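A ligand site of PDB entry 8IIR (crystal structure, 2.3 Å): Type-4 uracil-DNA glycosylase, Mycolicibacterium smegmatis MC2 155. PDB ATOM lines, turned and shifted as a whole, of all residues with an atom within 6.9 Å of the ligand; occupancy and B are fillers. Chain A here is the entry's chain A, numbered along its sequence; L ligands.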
ATOM      1  N   GLY A   2     -13.103  20.652  16.860  1.00  0.00           N
ATOM      2  CA  GLY A   2     -12.598  19.524  16.099  1.00  0.00           C
ATOM      3  C   GLY A   2     -11.243  19.805  15.474  1.00  0.00           C
ATOM      4  O   GLY A   2     -10.323  20.334  16.113  1.00  0.00           O
ATOM      5  N   ALA A   3     -11.115  19.445  14.194  1.00  0.00           N
ATOM      6  CA  ALA A   3      -9.872  19.563  13.447  1.00  0.00           C
ATOM      7  C   ALA A   3      -9.660  20.954  12.849  1.00  0.00           C
ATOM      8  O   ALA A   3      -8.626  21.163  12.206  1.00  0.00           O
ATOM      9  CB  ALA A   3      -9.826  18.521  12.328  1.00  0.00           C
ATOM     10  N   PHE A   6      -6.433  22.786  13.152  1.00  0.00           N
ATOM     11  CA  PHE A   6      -5.304  22.058  12.570  1.00  0.00           C
ATOM     12  C   PHE A   6      -5.261  22.169  11.052  1.00  0.00           C
ATOM     13  O   PHE A   6      -4.258  21.770  10.453  1.00  0.00           O
ATOM     14  CB  PHE A   6      -5.350  20.584  12.980  1.00  0.00           C
ATOM     15  CG  PHE A   6      -5.214  20.350  14.458  1.00  0.00           C
ATOM     16  CD1 PHE A   6      -3.974  20.377  15.064  1.00  0.00           C
ATOM     17  CD2 PHE A   6      -6.337  20.112  15.230  1.00  0.00           C
ATOM     18  CE1 PHE A   6      -3.845  20.165  16.426  1.00  0.00           C
ATOM     19  CE2 PHE A   6      -6.216  19.904  16.591  1.00  0.00           C
ATOM     20  CZ  PHE A   6      -4.975  19.932  17.187  1.00  0.00           C
ATOM     21  N   ALA A  20      -2.505  17.203   8.143  1.00  0.00           N
ATOM     22  CA  ALA A  20      -3.377  16.180   8.716  1.00  0.00           C
ATOM     23  C   ALA A  20      -2.590  15.175   9.552  1.00  0.00           C
ATOM     24  O   ALA A  20      -3.134  14.592  10.485  1.00  0.00           O
ATOM     25  CB  ALA A  20      -4.163  15.473   7.617  1.00  0.00           C
ATOM     26  N   GLY A  21      -1.317  14.970   9.222  1.00  0.00           N
ATOM     27  CA  GLY A  21      -0.461  14.127  10.033  1.00  0.00           C
ATOM     28  C   GLY A  21      -0.257  14.643  11.442  1.00  0.00           C
ATOM     29  O   GLY A  21       0.075  13.862  12.343  1.00  0.00           O
ATOM     30  N   GLU A  22      -0.458  15.942  11.662  1.00  0.00           N
ATOM     31  CA  GLU A  22      -0.337  16.564  12.971  1.00  0.00           C
ATOM     32  C   GLU A  22      -1.677  16.785  13.646  1.00  0.00           C
ATOM     33  O   GLU A  22      -1.720  17.393  14.723  1.00  0.00           O
ATOM     34  CB  GLU A  22       0.388  17.912  12.862  1.00  0.00           C
ATOM     35  CG  GLU A  22       1.625  17.876  11.992  1.00  0.00           C
ATOM     36  CD  GLU A  22       2.876  17.593  12.793  1.00  0.00           C
ATOM     37  OE1 GLU A  22       3.818  18.404  12.726  1.00  0.00           O
ATOM     38  OE2 GLU A  22       2.913  16.544  13.476  1.00  0.00           O
ATOM     39  N   CYS A  23      -2.777  16.334  13.056  1.00  0.00           N
ATOM     40  CA  CYS A  23      -4.096  16.646  13.586  1.00  0.00           C
ATOM     41  C   CYS A  23      -4.344  15.900  14.891  1.00  0.00           C
ATOM     42  O   CYS A  23      -4.032  14.715  15.030  1.00  0.00           O
ATOM     43  CB  CYS A  23      -5.183  16.292  12.579  1.00  0.00           C
ATOM     44  SG  CYS A  23      -6.866  16.759  13.091  1.00  0.00           S
ATOM     45  N   ARG A  24      -4.932  16.612  15.858  1.00  0.00           N
ATOM     46  CA  ARG A  24      -5.438  16.029  17.092  1.00  0.00           C
ATOM     47  C   ARG A  24      -6.915  16.377  17.280  1.00  0.00           C
ATOM     48  O   ARG A  24      -7.399  16.471  18.409  1.00  0.00           O
ATOM     49  CB  ARG A  24      -4.620  16.488  18.290  1.00  0.00           C
ATOM     50  CG  ARG A  24      -3.116  16.252  18.156  1.00  0.00           C
ATOM     51  CD  ARG A  24      -2.386  16.509  19.466  1.00  0.00           C
ATOM     52  NE  ARG A  24      -2.676  17.836  20.005  1.00  0.00           N
ATOM     53  CZ  ARG A  24      -2.092  18.954  19.587  1.00  0.00           C
ATOM     54  NH1 ARG A  24      -1.190  18.953  18.628  1.00  0.00           N
ATOM     55  NH2 ARG A  24      -2.424  20.108  20.158  1.00  0.00           N
ATOM     56  N   GLY A  25      -7.638  16.557  16.160  1.00  0.00           N
ATOM     57  CA  GLY A  25      -8.999  17.072  16.233  1.00  0.00           C
ATOM     58  C   GLY A  25      -9.953  16.163  16.986  1.00  0.00           C
ATOM     59  O   GLY A  25     -10.962  16.631  17.515  1.00  0.00           O
ATOM     60  N   CYS A  26      -9.657  14.869  17.032  1.00  0.00           N
ATOM     61  CA  CYS A  26     -10.389  13.921  17.864  1.00  0.00           C
ATOM     62  C   CYS A  26      -9.381  12.933  18.429  1.00  0.00           C
ATOM     63  O   CYS A  26      -8.165  13.134  18.312  1.00  0.00           O
ATOM     64  CB  CYS A  26     -11.524  13.256  17.067  1.00  0.00           C
ATOM     65  SG  CYS A  26     -11.002  12.005  15.868  1.00  0.00           S
ATOM     66  N   GLY A  27      -9.859  11.850  19.033  1.00  0.00           N
ATOM     67  CA  GLY A  27      -8.963  10.916  19.694  1.00  0.00           C
ATOM     68  C   GLY A  27      -8.341   9.857  18.813  1.00  0.00           C
ATOM     69  O   GLY A  27      -7.461   9.118  19.262  1.00  0.00           O
ATOM     70  N   LEU A  28      -8.772   9.763  17.551  1.00  0.00           N
ATOM     71  CA  LEU A  28      -8.399   8.626  16.712  1.00  0.00           C
ATOM     72  C   LEU A  28      -6.932   8.626  16.300  1.00  0.00           C
ATOM     73  O   LEU A  28      -6.416   7.589  15.889  1.00  0.00           O
ATOM     74  CB  LEU A  28      -9.298   8.581  15.471  1.00  0.00           C
ATOM     75  CG  LEU A  28     -10.776   8.336  15.795  1.00  0.00           C
ATOM     76  CD1 LEU A  28     -11.637   8.312  14.534  1.00  0.00           C
ATOM     77  CD2 LEU A  28     -10.953   7.052  16.584  1.00  0.00           C
ATOM     78  N   TYR A  29      -6.234   9.763  16.412  1.00  0.00           N
ATOM     79  CA  TYR A  29      -4.830   9.801  16.005  1.00  0.00           C
ATOM     80  C   TYR A  29      -3.931   8.987  16.923  1.00  0.00           C
ATOM     81  O   TYR A  29      -2.817   8.641  16.522  1.00  0.00           O
ATOM     82  CB  TYR A  29      -4.329  11.255  15.956  1.00  0.00           C
ATOM     83  CG  TYR A  29      -4.102  11.845  17.323  1.00  0.00           C
ATOM     84  CD1 TYR A  29      -5.164  12.380  18.048  1.00  0.00           C
ATOM     85  CD2 TYR A  29      -2.838  11.866  17.905  1.00  0.00           C
ATOM     86  CE1 TYR A  29      -4.964  12.923  19.302  1.00  0.00           C
ATOM     87  CE2 TYR A  29      -2.633  12.397  19.159  1.00  0.00           C
ATOM     88  CZ  TYR A  29      -3.711  12.931  19.859  1.00  0.00           C
ATOM     89  OH  TYR A  29      -3.533  13.474  21.107  1.00  0.00           O
ATOM     90  N   ARG A  30      -4.359   8.691  18.151  1.00  0.00           N
ATOM     91  CA  ARG A  30      -3.484   8.048  19.164  1.00  0.00           C
ATOM     92  C   ARG A  30      -3.128   6.596  18.813  1.00  0.00           C
ATOM     93  O   ARG A  30      -1.944   6.267  18.795  1.00  0.00           O
ATOM     94  CB  ARG A  30      -4.100   8.143  20.558  1.00  0.00           C
ATOM     95  CG  ARG A  30      -4.471   9.555  20.986  1.00  0.00           C
ATOM     96  CD  ARG A  30      -4.791   9.601  22.457  1.00  0.00           C
ATOM     97  NE  ARG A  30      -6.118  10.112  22.798  1.00  0.00           N
ATOM     98  CZ  ARG A  30      -7.257   9.416  22.735  1.00  0.00           C
ATOM     99  NH1 ARG A  30      -7.255   8.167  22.319  1.00  0.00           N
ATOM    100  NH2 ARG A  30      -8.394   9.986  23.099  1.00  0.00           N
ATOM    101  N   ALA A  35      -2.116   9.421   9.657  1.00  0.00           N
ATOM    102  CA  ALA A  35      -3.347   9.918   9.038  1.00  0.00           C
ATOM    103  C   ALA A  35      -3.372   9.445   7.576  1.00  0.00           C
ATOM    104  O   ALA A  35      -2.323   9.427   6.946  1.00  0.00           O
ATOM    105  CB  ALA A  35      -3.402  11.418   9.131  1.00  0.00           C
ATOM    106  N   ALA A  91     -14.234   9.980   5.141  1.00  0.00           N
ATOM    107  CA  ALA A  91     -14.887  10.952   6.030  1.00  0.00           C
ATOM    108  C   ALA A  91     -14.013  11.288   7.228  1.00  0.00           C
ATOM    109  O   ALA A  91     -13.896  12.460   7.609  1.00  0.00           O
ATOM    110  CB  ALA A  91     -16.234  10.409   6.499  1.00  0.00           C
ATOM    111  N   VAL A  92     -13.414  10.285   7.868  1.00  0.00           N
ATOM    112  CA  VAL A  92     -12.429  10.512   8.913  1.00  0.00           C
ATOM    113  C   VAL A  92     -11.112   9.929   8.431  1.00  0.00           C
ATOM    114  O   VAL A  92     -11.088   8.986   7.632  1.00  0.00           O
ATOM    115  CB  VAL A  92     -12.859   9.919  10.281  1.00  0.00           C
ATOM    116  CG1 VAL A  92     -14.325  10.214  10.553  1.00  0.00           C
ATOM    117  CG2 VAL A  92     -12.578   8.430  10.344  1.00  0.00           C
ATOM    118  N   LYS A  93     -10.026  10.564   8.871  1.00  0.00           N
ATOM    119  CA  LYS A  93      -8.675  10.240   8.328  1.00  0.00           C
ATOM    120  C   LYS A  93      -7.845   9.308   9.211  1.00  0.00           C
ATOM    121  O   LYS A  93      -6.809   8.861   8.753  1.00  0.00           O
ATOM    122  CB  LYS A  93      -7.939  11.554   8.065  1.00  0.00           C
ATOM    123  CG  LYS A  93      -8.705  12.615   7.300  1.00  0.00           C
ATOM    124  CD  LYS A  93      -8.964  12.236   5.862  1.00  0.00           C
ATOM    125  CE  LYS A  93      -9.111  13.444   4.961  1.00  0.00           C
ATOM    126  NZ  LYS A  93     -10.529  13.727   4.654  1.00  0.00           N
ATOM    127  N   HIS A  94      -8.293   9.064  10.436  1.00  0.00           N
ATOM    128  CA  HIS A  94      -7.582   8.069  11.273  1.00  0.00           C
ATOM    129  C   HIS A  94      -8.359   6.769  11.359  1.00  0.00           C
ATOM    130  O   HIS A  94      -9.572   6.830  11.542  1.00  0.00           O
ATOM    131  CB  HIS A  94      -7.095   8.621  12.615  1.00  0.00           C
ATOM    132  CG  HIS A  94      -5.834   9.393  12.508  1.00  0.00           C
ATOM    133  ND1 HIS A  94      -5.842  10.732  12.387  1.00  0.00           N
ATOM    134  CD2 HIS A  94      -4.551   9.010  12.493  1.00  0.00           C
ATOM    135  CE1 HIS A  94      -4.608  11.178  12.329  1.00  0.00           C
ATOM    136  NE2 HIS A  94      -3.812  10.144  12.388  1.00  0.00           N
ATOM    137  N   PHE A  95      -7.675   5.645  11.248  1.00  0.00           N
ATOM    138  CA  PHE A  95      -8.279   4.315  11.401  1.00  0.00           C
ATOM    139  C   PHE A  95      -8.716   4.051  12.856  1.00  0.00           C
ATOM    140  O   PHE A  95      -7.869   4.110  13.742  1.00  0.00           O
ATOM    141  CB  PHE A  95      -7.259   3.252  11.001  1.00  0.00           C
ATOM    142  CG  PHE A  95      -7.612   1.790  11.121  1.00  0.00           C
ATOM    143  CD1 PHE A  95      -8.886   1.318  10.835  1.00  0.00           C
ATOM    144  CD2 PHE A  95      -6.649   0.857  11.469  1.00  0.00           C
ATOM    145  CE1 PHE A  95      -9.180  -0.032  10.926  1.00  0.00           C
ATOM    146  CE2 PHE A  95      -6.954  -0.490  11.567  1.00  0.00           C
ATOM    147  CZ  PHE A  95      -8.217  -0.934  11.285  1.00  0.00           C
ATOM    148  N   GLU A 115     -16.844  12.215  15.750  1.00  0.00           N
ATOM    149  CA  GLU A 115     -15.545  12.075  15.026  1.00  0.00           C
ATOM    150  C   GLU A 115     -15.733  12.525  13.567  1.00  0.00           C
ATOM    151  O   GLU A 115     -14.873  13.199  13.077  1.00  0.00           O
ATOM    152  CB  GLU A 115     -14.957  10.682  15.260  1.00  0.00           C
ATOM    153  CG  GLU A 115     -14.614  10.366  16.706  1.00  0.00           C
ATOM    154  CD  GLU A 115     -14.573   8.891  17.036  1.00  0.00           C
ATOM    155  OE1 GLU A 115     -15.269   8.120  16.362  1.00  0.00           O
ATOM    156  OE2 GLU A 115     -13.848   8.512  17.960  1.00  0.00           O
ATOM    157  N   VAL A 117     -17.966  14.802  12.550  1.00  0.00           N
ATOM    158  CA  VAL A 117     -18.064  16.299  12.631  1.00  0.00           C
ATOM    159  C   VAL A 117     -16.675  16.904  12.882  1.00  0.00           C
ATOM    160  O   VAL A 117     -16.355  17.886  12.230  1.00  0.00           O
ATOM    161  CB  VAL A 117     -19.162  16.764  13.602  1.00  0.00           C
ATOM    162  CG1 VAL A 117     -19.125  18.268  13.834  1.00  0.00           C
ATOM    163  CG2 VAL A 117     -20.544  16.334  13.144  1.00  0.00           C
ATOM    164  N   ALA A 118     -15.866  16.264  13.711  1.00  0.00           N
ATOM    165  CA  ALA A 118     -14.495  16.727  14.002  1.00  0.00           C
ATOM    166  C   ALA A 118     -13.600  16.700  12.749  1.00  0.00           C
ATOM    167  O   ALA A 118     -12.899  17.663  12.573  1.00  0.00           O
ATOM    168  CB  ALA A 118     -13.930  15.950  15.153  1.00  0.00           C
ATOM    169  N   CYS A 119     -13.685  15.654  11.926  1.00  0.00           N
ATOM    170  CA  CYS A 119     -12.829  15.479  10.738  1.00  0.00           C
ATOM    171  C   CYS A 119     -13.356  16.252   9.515  1.00  0.00           C
ATOM    172  O   CYS A 119     -12.549  16.498   8.626  1.00  0.00           O
ATOM    173  CB  CYS A 119     -12.644  14.009  10.402  1.00  0.00           C
ATOM    174  SG  CYS A 119     -11.113  13.645   9.512  1.00  0.00           S
ATOM    175  N   ARG A 120     -14.636  16.604   9.508  1.00  0.00           N
ATOM    176  CA  ARG A 120     -15.291  17.348   8.383  1.00  0.00           C
ATOM    177  C   ARG A 120     -14.453  18.520   7.860  1.00  0.00           C
ATOM    178  O   ARG A 120     -14.391  18.647   6.660  1.00  0.00           O
ATOM    179  CB  ARG A 120     -16.768  17.661   8.643  1.00  0.00           C
ATOM    180  CG  ARG A 120     -17.613  17.643   7.376  1.00  0.00           C
ATOM    181  CD  ARG A 120     -19.107  17.728   7.598  1.00  0.00           C
ATOM    182  NE  ARG A 120     -19.537  18.533   8.736  1.00  0.00           N
ATOM    183  CZ  ARG A 120     -20.700  18.394   9.348  1.00  0.00           C
ATOM    184  NH1 ARG A 120     -21.575  17.500   8.941  1.00  0.00           N
ATOM    185  NH2 ARG A 120     -20.992  19.170  10.377  1.00  0.00           N
ATOM    186  N   PRO A 121     -13.847  19.401   8.692  1.00  0.00           N
ATOM    187  CA  PRO A 121     -12.950  20.445   8.189  1.00  0.00           C
ATOM    188  C   PRO A 121     -11.954  19.988   7.097  1.00  0.00           C
ATOM    189  O   PRO A 121     -11.821  20.701   6.153  1.00  0.00           O
ATOM    190  CB  PRO A 121     -12.313  21.035   9.449  1.00  0.00           C
ATOM    191  CG  PRO A 121     -13.332  20.824  10.532  1.00  0.00           C
ATOM    192  CD  PRO A 121     -14.063  19.561  10.135  1.00  0.00           C
ATOM    193  N   TRP A 122     -11.374  18.791   7.224  1.00  0.00           N
ATOM    194  CA  TRP A 122     -10.459  18.224   6.209  1.00  0.00           C
ATOM    195  C   TRP A 122     -11.212  17.943   4.902  1.00  0.00           C
ATOM    196  O   TRP A 122     -10.690  18.354   3.871  1.00  0.00           O
ATOM    197  CB  TRP A 122      -9.734  16.967   6.735  1.00  0.00           C
ATOM    198  CG  TRP A 122      -8.798  17.210   7.872  1.00  0.00           C
ATOM    199  CD1 TRP A 122      -8.890  16.702   9.128  1.00  0.00           C
ATOM    200  CD2 TRP A 122      -7.593  17.994   7.834  1.00  0.00           C
ATOM    201  NE1 TRP A 122      -7.834  17.123   9.881  1.00  0.00           N
ATOM    202  CE2 TRP A 122      -7.028  17.929   9.124  1.00  0.00           C
ATOM    203  CE3 TRP A 122      -6.951  18.764   6.853  1.00  0.00           C
ATOM    204  CZ2 TRP A 122      -5.854  18.600   9.455  1.00  0.00           C
ATOM    205  CZ3 TRP A 122      -5.789  19.407   7.180  1.00  0.00           C
ATOM    206  CH2 TRP A 122      -5.246  19.332   8.454  1.00  0.00           C
HETATM  207 FE1  LIG L   1      -9.730  13.426  11.586  1.00  0.00          FE
HETATM  208 FE2  LIG L   1      -9.649  12.916  14.279  1.00  0.00          FE
HETATM  209 FE3  LIG L   1      -7.927  14.744  13.179  1.00  0.00          FE
HETATM  210 FE4  LIG L   1      -7.602  12.083  12.664  1.00  0.00          FE
HETATM  211  S1  LIG L   1      -7.399  13.123  14.691  1.00  0.00           S
HETATM  212  S2  LIG L   1      -7.524  13.791  11.144  1.00  0.00           S
HETATM  213  S3  LIG L   1      -9.767  11.380  12.582  1.00  0.00           S
HETATM  214  S4  LIG L   1     -10.203  14.881  13.285  1.00  0.00           S
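The backbone NH (N) of His 94 lies close to a sulfur (S3) of the ligand, 3.5 Å away. ND1 of His 94 is bound to FE4 of the ligand, 2.2 Å away. N of Cys 26 sits close to S1 of the ligand (3.7 Å). An iron atom (FE2) of the ligand is bound by the side-chain sulfur of Cys 26, at 2.3 Å. FE3 of the ligand is bound by SG of Cys 23, 2.3 Å away. The side-chain sulfur (SG) of Cys 119 is bound to an iron atom (FE1) of the ligand, 2.5 Å away. S1 of the ligand lies close to N of Gly 25. A sulfur (S2) of the ligand lies close to the indole nitrogen of Trp 122 (3.6 Å).
Ala 3 touches the ligand. Tyr 29 touches the ligand (CB to S1, 3.8 Å). Lys 93 touches the ligand. Ala 118 touches the ligand. Ten residues have an atom within 4 Å of the ligand: Ala 3, Cys 23, Gly 25, Cys 26, Tyr 29, Lys 93, His 94, Ala 118, Cys 119 and Trp 122. Along chain A the residues within 4 Å of the ligand span positions 3 to 122. The nearest printed residue that does not touch the ligand is Leu 28 (4.05 Å).
A ring nitrogen (NE2) of His 94 sits at hydrogen-bond distance from the backbone NH (N) of Ala 35 (3.3 Å). The backbone NH (N) of Leu 28 sits close to the side-chain sulfur (SG) of Cys 26. The side-chain sulfur (SG) of Cys 23 lies close to the backbone NH (N) of Gly 25, 3.2 Å away. SG of Cys 23 lies close to NE1 of Trp 122, 3.4 Å away. The side-chain sulfur (SG) of Cys 119 sits close to the backbone NH (N) of Lys 93 (3.3 Å). SG of Cys 119 lies close to O of Ala 91, 3.6 Å away. The backbone NH (N) of Ala 3 sits at hydrogen-bond distance from the backbone carbonyl oxygen (O) of Ala 118 (3.0 Å).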
